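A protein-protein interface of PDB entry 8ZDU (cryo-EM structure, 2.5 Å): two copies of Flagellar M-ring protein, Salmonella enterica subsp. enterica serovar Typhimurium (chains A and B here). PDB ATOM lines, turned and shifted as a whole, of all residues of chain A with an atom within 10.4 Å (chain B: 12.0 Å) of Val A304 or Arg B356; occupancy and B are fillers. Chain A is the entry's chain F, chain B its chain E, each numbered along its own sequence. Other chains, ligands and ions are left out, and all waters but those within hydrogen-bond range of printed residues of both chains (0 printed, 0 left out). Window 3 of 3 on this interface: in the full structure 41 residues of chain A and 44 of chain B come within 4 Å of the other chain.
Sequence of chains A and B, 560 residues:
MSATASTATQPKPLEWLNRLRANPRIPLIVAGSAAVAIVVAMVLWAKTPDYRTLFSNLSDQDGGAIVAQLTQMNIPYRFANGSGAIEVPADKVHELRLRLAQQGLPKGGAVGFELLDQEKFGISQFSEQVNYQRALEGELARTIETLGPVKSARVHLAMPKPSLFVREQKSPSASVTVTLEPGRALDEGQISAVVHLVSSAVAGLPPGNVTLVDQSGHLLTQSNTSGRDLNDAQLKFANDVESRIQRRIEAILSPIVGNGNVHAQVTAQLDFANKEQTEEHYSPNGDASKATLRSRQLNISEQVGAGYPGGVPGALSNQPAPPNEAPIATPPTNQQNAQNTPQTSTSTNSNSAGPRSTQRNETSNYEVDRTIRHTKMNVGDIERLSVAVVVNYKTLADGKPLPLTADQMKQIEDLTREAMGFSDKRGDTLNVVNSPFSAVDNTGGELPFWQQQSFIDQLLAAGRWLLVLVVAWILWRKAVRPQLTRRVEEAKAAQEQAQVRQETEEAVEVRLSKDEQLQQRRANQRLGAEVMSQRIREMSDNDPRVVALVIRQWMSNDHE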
ATOM      1  N   SER A 301     -14.410   6.088 -18.790  1.00  0.00           N
ATOM      2  CA  SER A 301     -13.770   5.084 -19.627  1.00  0.00           C
ATOM      3  C   SER A 301     -13.793   5.554 -21.074  1.00  0.00           C
ATOM      4  O   SER A 301     -14.680   6.308 -21.482  1.00  0.00           O
ATOM      5  CB  SER A 301     -14.461   3.720 -19.503  1.00  0.00           C
ATOM      6  OG  SER A 301     -13.865   2.767 -20.366  1.00  0.00           O
ATOM      7  N   GLU A 302     -12.809   5.100 -21.848  1.00  0.00           N
ATOM      8  CA  GLU A 302     -12.702   5.501 -23.244  1.00  0.00           C
ATOM      9  C   GLU A 302     -11.821   4.509 -23.989  1.00  0.00           C
ATOM     10  O   GLU A 302     -10.666   4.295 -23.614  1.00  0.00           O
ATOM     11  CB  GLU A 302     -12.130   6.918 -23.374  1.00  0.00           C
ATOM     12  CG  GLU A 302     -11.684   7.281 -24.780  1.00  0.00           C
ATOM     13  CD  GLU A 302     -11.157   8.699 -24.875  1.00  0.00           C
ATOM     14  OE1 GLU A 302     -11.509   9.402 -25.845  1.00  0.00           O
ATOM     15  OE2 GLU A 302     -10.389   9.111 -23.980  1.00  0.00           O
ATOM     16  N   GLN A 303     -12.375   3.911 -25.044  1.00  0.00           N
ATOM     17  CA  GLN A 303     -11.623   3.037 -25.934  1.00  0.00           C
ATOM     18  C   GLN A 303     -11.578   3.666 -27.318  1.00  0.00           C
ATOM     19  O   GLN A 303     -12.580   4.207 -27.796  1.00  0.00           O
ATOM     20  CB  GLN A 303     -12.229   1.622 -26.041  1.00  0.00           C
ATOM     21  CG  GLN A 303     -12.547   0.902 -24.728  1.00  0.00           C
ATOM     22  CD  GLN A 303     -13.812   1.397 -24.047  1.00  0.00           C
ATOM     23  OE1 GLN A 303     -13.978   2.586 -23.791  1.00  0.00           O
ATOM     24  NE2 GLN A 303     -14.717   0.471 -23.750  1.00  0.00           N
ATOM     25  N   VAL A 304     -10.415   3.595 -27.958  1.00  0.00           N
ATOM     26  CA  VAL A 304     -10.245   4.143 -29.298  1.00  0.00           C
ATOM     27  C   VAL A 304      -9.652   3.092 -30.227  1.00  0.00           C
ATOM     28  O   VAL A 304      -9.954   1.904 -30.111  1.00  0.00           O
ATOM     29  CB  VAL A 304      -9.368   5.407 -29.279  1.00  0.00           C
ATOM     30  CG1 VAL A 304      -8.982   5.804 -30.695  1.00  0.00           C
ATOM     31  CG2 VAL A 304     -10.094   6.548 -28.582  1.00  0.00           C
ATOM     32  N   PRO A 355     -13.934   3.344 -34.828  1.00  0.00           N
ATOM     33  CA  PRO A 355     -14.538   2.776 -33.620  1.00  0.00           C
ATOM     34  C   PRO A 355     -14.174   3.555 -32.361  1.00  0.00           C
ATOM     35  O   PRO A 355     -13.034   3.486 -31.902  1.00  0.00           O
ATOM     36  CB  PRO A 355     -13.957   1.362 -33.573  1.00  0.00           C
ATOM     37  CG  PRO A 355     -13.676   1.032 -34.996  1.00  0.00           C
ATOM     38  CD  PRO A 355     -13.240   2.322 -35.632  1.00  0.00           C
ATOM     39  N   ARG A 356     -15.139   4.292 -31.812  1.00  0.00           N
ATOM     40  CA  ARG A 356     -14.923   5.093 -30.615  1.00  0.00           C
ATOM     41  C   ARG A 356     -15.986   4.747 -29.585  1.00  0.00           C
ATOM     42  O   ARG A 356     -17.177   4.717 -29.906  1.00  0.00           O
ATOM     43  CB  ARG A 356     -14.964   6.592 -30.936  1.00  0.00           C
ATOM     44  CG  ARG A 356     -13.832   7.390 -30.315  1.00  0.00           C
ATOM     45  CD  ARG A 356     -14.007   8.879 -30.563  1.00  0.00           C
ATOM     46  NE  ARG A 356     -13.343   9.684 -29.546  1.00  0.00           N
ATOM     47  CZ  ARG A 356     -13.960  10.252 -28.519  1.00  0.00           C
ATOM     48  NH1 ARG A 356     -15.264  10.125 -28.341  1.00  0.00           N
ATOM     49  NH2 ARG A 356     -13.249  10.965 -27.649  1.00  0.00           N
ATOM     50  N   SER A 357     -15.552   4.488 -28.355  1.00  0.00           N
ATOM     51  CA  SER A 357     -16.446   4.174 -27.249  1.00  0.00           C
ATOM     52  C   SER A 357     -16.166   5.111 -26.084  1.00  0.00           C
ATOM     53  O   SER A 357     -15.006   5.380 -25.756  1.00  0.00           O
ATOM     54  CB  SER A 357     -16.286   2.717 -26.801  1.00  0.00           C
ATOM     55  OG  SER A 357     -16.694   1.822 -27.822  1.00  0.00           O
ATOM     56  N   THR A 358     -17.233   5.608 -25.461  1.00  0.00           N
ATOM     57  CA  THR A 358     -17.120   6.517 -24.331  1.00  0.00           C
ATOM     58  C   THR A 358     -18.183   6.172 -23.301  1.00  0.00           C
ATOM     59  O   THR A 358     -19.334   5.901 -23.654  1.00  0.00           O
ATOM     60  CB  THR A 358     -17.268   7.980 -24.772  1.00  0.00           C
ATOM     61  OG1 THR A 358     -16.369   8.247 -25.856  1.00  0.00           O
ATOM     62  CG2 THR A 358     -16.952   8.922 -23.621  1.00  0.00           C
ATOM     63  N   GLN A 359     -17.792   6.183 -22.028  1.00  0.00           N
ATOM     64  CA  GLN A 359     -18.702   5.890 -20.929  1.00  0.00           C
ATOM     65  C   GLN A 359     -18.368   6.799 -19.758  1.00  0.00           C
ATOM     66  O   GLN A 359     -17.192   6.988 -19.433  1.00  0.00           O
ATOM     67  CB  GLN A 359     -18.608   4.420 -20.507  1.00  0.00           C
ATOM     68  CG  GLN A 359     -19.628   4.006 -19.462  1.00  0.00           C
ATOM     69  CD  GLN A 359     -19.568   2.525 -19.146  1.00  0.00           C
ATOM     70  OE1 GLN A 359     -18.809   1.778 -19.762  1.00  0.00           O
ATOM     71  NE2 GLN A 359     -20.372   2.093 -18.181  1.00  0.00           N
ATOM     72  N   ILE B 300      -6.144   4.611 -11.869  1.00  0.00           N
ATOM     73  CA  ILE B 300      -5.839   5.018 -13.236  1.00  0.00           C
ATOM     74  C   ILE B 300      -5.255   3.830 -13.987  1.00  0.00           C
ATOM     75  O   ILE B 300      -4.392   3.116 -13.465  1.00  0.00           O
ATOM     76  CB  ILE B 300      -4.863   6.214 -13.274  1.00  0.00           C
ATOM     77  CG1 ILE B 300      -5.376   7.358 -12.395  1.00  0.00           C
ATOM     78  CG2 ILE B 300      -4.657   6.693 -14.702  1.00  0.00           C
ATOM     79  CD1 ILE B 300      -4.457   8.557 -12.358  1.00  0.00           C
ATOM     80  N   SER B 301      -5.731   3.619 -15.213  1.00  0.00           N
ATOM     81  CA  SER B 301      -5.224   2.566 -16.080  1.00  0.00           C
ATOM     82  C   SER B 301      -5.090   3.106 -17.495  1.00  0.00           C
ATOM     83  O   SER B 301      -5.816   4.020 -17.897  1.00  0.00           O
ATOM     84  CB  SER B 301      -6.139   1.333 -16.068  1.00  0.00           C
ATOM     85  OG  SER B 301      -5.664   0.338 -16.958  1.00  0.00           O
ATOM     86  N   GLU B 302      -4.156   2.532 -18.252  1.00  0.00           N
ATOM     87  CA  GLU B 302      -3.909   2.979 -19.615  1.00  0.00           C
ATOM     88  C   GLU B 302      -3.167   1.893 -20.378  1.00  0.00           C
ATOM     89  O   GLU B 302      -2.086   1.467 -19.966  1.00  0.00           O
ATOM     90  CB  GLU B 302      -3.103   4.284 -19.634  1.00  0.00           C
ATOM     91  CG  GLU B 302      -2.527   4.638 -20.995  1.00  0.00           C
ATOM     92  CD  GLU B 302      -1.767   5.950 -20.983  1.00  0.00           C
ATOM     93  OE1 GLU B 302      -1.945   6.752 -21.924  1.00  0.00           O
ATOM     94  OE2 GLU B 302      -0.990   6.179 -20.032  1.00  0.00           O
ATOM     95  N   GLN B 303      -3.755   1.451 -21.490  1.00  0.00           N
ATOM     96  CA  GLN B 303      -3.115   0.511 -22.397  1.00  0.00           C
ATOM     97  C   GLN B 303      -2.891   1.193 -23.737  1.00  0.00           C
ATOM     98  O   GLN B 303      -3.761   1.920 -24.226  1.00  0.00           O
ATOM     99  CB  GLN B 303      -3.941  -0.775 -22.614  1.00  0.00           C
ATOM    100  CG  GLN B 303      -4.444  -1.497 -21.362  1.00  0.00           C
ATOM    101  CD  GLN B 303      -5.644  -0.830 -20.709  1.00  0.00           C
ATOM    102  OE1 GLN B 303      -5.623   0.357 -20.391  1.00  0.00           O
ATOM    103  NE2 GLN B 303      -6.705  -1.603 -20.508  1.00  0.00           N
ATOM    104  N   VAL B 304      -1.724   0.958 -24.328  1.00  0.00           N
ATOM    105  CA  VAL B 304      -1.393   1.537 -25.625  1.00  0.00           C
ATOM    106  C   VAL B 304      -0.934   0.450 -26.588  1.00  0.00           C
ATOM    107  O   VAL B 304      -1.436  -0.674 -26.556  1.00  0.00           O
ATOM    108  CB  VAL B 304      -0.320   2.632 -25.492  1.00  0.00           C
ATOM    109  CG1 VAL B 304       0.203   3.029 -26.863  1.00  0.00           C
ATOM    110  CG2 VAL B 304      -0.881   3.842 -24.761  1.00  0.00           C
ATOM    111  N   PRO B 355      -4.862   1.661 -31.350  1.00  0.00           N
ATOM    112  CA  PRO B 355      -5.617   1.142 -30.206  1.00  0.00           C
ATOM    113  C   PRO B 355      -5.195   1.783 -28.888  1.00  0.00           C
ATOM    114  O   PRO B 355      -4.109   1.498 -28.383  1.00  0.00           O
ATOM    115  CB  PRO B 355      -5.283  -0.351 -30.217  1.00  0.00           C
ATOM    116  CG  PRO B 355      -4.985  -0.649 -31.644  1.00  0.00           C
ATOM    117  CD  PRO B 355      -4.306   0.579 -32.181  1.00  0.00           C
ATOM    118  N   ARG B 356      -6.052   2.644 -28.339  1.00  0.00           N
ATOM    119  CA  ARG B 356      -5.770   3.333 -27.088  1.00  0.00           C
ATOM    120  C   ARG B 356      -6.928   3.120 -26.128  1.00  0.00           C
ATOM    121  O   ARG B 356      -8.089   3.310 -26.502  1.00  0.00           O
ATOM    122  CB  ARG B 356      -5.542   4.831 -27.320  1.00  0.00           C
ATOM    123  CG  ARG B 356      -4.328   5.394 -26.603  1.00  0.00           C
ATOM    124  CD  ARG B 356      -4.239   6.902 -26.770  1.00  0.00           C
ATOM    125  NE  ARG B 356      -3.504   7.529 -25.679  1.00  0.00           N
ATOM    126  CZ  ARG B 356      -4.073   8.140 -24.647  1.00  0.00           C
ATOM    127  NH1 ARG B 356      -5.387   8.228 -24.535  1.00  0.00           N
ATOM    128  NH2 ARG B 356      -3.301   8.676 -23.706  1.00  0.00           N
ATOM    129  N   SER B 357      -6.611   2.728 -24.897  1.00  0.00           N
ATOM    130  CA  SER B 357      -7.603   2.515 -23.853  1.00  0.00           C
ATOM    131  C   SER B 357      -7.232   3.330 -22.622  1.00  0.00           C
ATOM    132  O   SER B 357      -6.063   3.381 -22.229  1.00  0.00           O
ATOM    133  CB  SER B 357      -7.712   1.031 -23.486  1.00  0.00           C
ATOM    134  OG  SER B 357      -8.208   0.272 -24.575  1.00  0.00           O
ATOM    135  N   THR B 358      -8.233   3.967 -22.019  1.00  0.00           N
ATOM    136  CA  THR B 358      -8.031   4.785 -20.833  1.00  0.00           C
ATOM    137  C   THR B 358      -9.191   4.574 -19.873  1.00  0.00           C
ATOM    138  O   THR B 358     -10.350   4.520 -20.292  1.00  0.00           O
ATOM    139  CB  THR B 358      -7.908   6.272 -21.192  1.00  0.00           C
ATOM    140  OG1 THR B 358      -6.920   6.439 -22.217  1.00  0.00           O
ATOM    141  CG2 THR B 358      -7.502   7.087 -19.974  1.00  0.00           C
ATOM    142  N   GLN B 359      -8.872   4.452 -18.586  1.00  0.00           N
ATOM    143  CA  GLN B 359      -9.874   4.262 -17.548  1.00  0.00           C
ATOM    144  C   GLN B 359      -9.457   5.041 -16.311  1.00  0.00           C
ATOM    145  O   GLN B 359      -8.286   5.010 -15.924  1.00  0.00           O
ATOM    146  CB  GLN B 359     -10.050   2.777 -17.210  1.00  0.00           C
ATOM    147  CG  GLN B 359     -11.180   2.490 -16.238  1.00  0.00           C
ATOM    148  CD  GLN B 359     -11.385   1.006 -16.009  1.00  0.00           C
ATOM    149  OE1 GLN B 359     -10.728   0.174 -16.633  1.00  0.00           O
ATOM    150  NE2 GLN B 359     -12.299   0.667 -15.107  1.00  0.00           N
ATOM    151  N   ARG B 360     -10.412   5.736 -15.696  1.00  0.00           N
ATOM    152  CA  ARG B 360     -10.140   6.554 -14.522  1.00  0.00           C
ATOM    153  C   ARG B 360     -11.311   6.464 -13.557  1.00  0.00           C
ATOM    154  O   ARG B 360     -12.448   6.771 -13.927  1.00  0.00           O
ATOM    155  CB  ARG B 360      -9.888   8.014 -14.913  1.00  0.00           C
ATOM    156  CG  ARG B 360      -9.679   8.947 -13.735  1.00  0.00           C
ATOM    157  CD  ARG B 360      -9.013  10.242 -14.170  1.00  0.00           C
ATOM    158  NE  ARG B 360      -9.014  11.240 -13.107  1.00  0.00           N
ATOM    159  CZ  ARG B 360      -7.945  11.923 -12.720  1.00  0.00           C
ATOM    160  NH1 ARG B 360      -6.765  11.741 -13.290  1.00  0.00           N
ATOM    161  NH2 ARG B 360      -8.063  12.810 -11.737  1.00  0.00           N
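N of Thr B358 sits at hydrogen-bond distance from O of Glu A302. The backbone NH (N) of Val A304 sits at hydrogen-bond distance from the backbone carbonyl oxygen (O) of Arg B356 (2.8 Å).
Val A304 touches just one residue of chain B: Arg B356 (2.8 Å). Of the printed residues of chain A, Arg B356 touches Glu A302 (3.99 Å), Gln A303 (3.6 Å) and Val A304 (2.8 Å). Of the printed residues of chain B, Gln A303 touches Arg B356 (3.6 Å). No residue of chain B comes within 4 Å of Arg A356. Ser A357 touches none of the printed residues of chain B. No residue of chain A comes within 4 Å of Val B304. No residue of chain A comes within 4 Å of Pro B355. Ser B357 touches one residue of chain A. Of the printed residues of chain A, Thr B358 touches Ser A301 (3.5 Å) and Glu A302 (2.9 Å). Printed residues of chain B within 4 Å of Glu A302: Arg B356 (3.99 Å), Ser B357 (3.6 Å) and Thr B358 (2.9 Å). Printed residues of chain B within 4 Å of Ser A301: Thr B358 (3.5 Å). The nearest printed residue of chain B that does not touch Glu A302 is Gln B359 (5.2 Å).
Among the printed residues, merely in contact across the chains: Ser A301 with Thr B358 (3.5 Å), Glu A302 with Arg B356 (3.99 Å), Glu A302 with Ser B357 (3.6 Å) and Gln A303 with Arg B356 (3.6 Å).
Glu A302 touches Arg B356, but with the chains exchanged Arg A356 does not touch Glu B302 (13.4 Å). Glu A302 touches Ser B357, but with the chains exchanged Ser A357 does not touch Glu B302 (12.9 Å). Glu A302 touches Thr B358, but with the chains exchanged Thr A358 does not touch Glu B302 (14.5 Å). Val A304 touches Arg B356, but with the chains exchanged Arg A356 does not touch Val B304 (14.5 Å).
The guanidinium group of Arg A356 lies within salt-bridge range of the side-chain carboxylate of Glu A302, at 3.0 Å. The backbone NH of Ser A301 is in hydrogen-bond range of the backbone carbonyl oxygen of Gln A359. The side-chain amide oxygen of Gln A303 sits at hydrogen-bond distance from the side-chain hydroxyl of Ser A301, 3.4 Å away. The side-chain carboxylate (OE1) of Glu B302 is in salt-bridge range of the guanidinium group (NH2) of Arg B356. NH1 of Arg B356 is in hydrogen-bond range of OG1 of Thr B358, at 3.3 Å. The backbone NH (N) of Ser A357 is in hydrogen-bond range of the backbone carbonyl oxygen (O) of Gln A303 (3.0 Å).
Of the 11 printed residues of chain B, 3 touch a printed residue of chain A. Of the 9 printed residues of chain A, 4 touch a printed residue of chain B.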
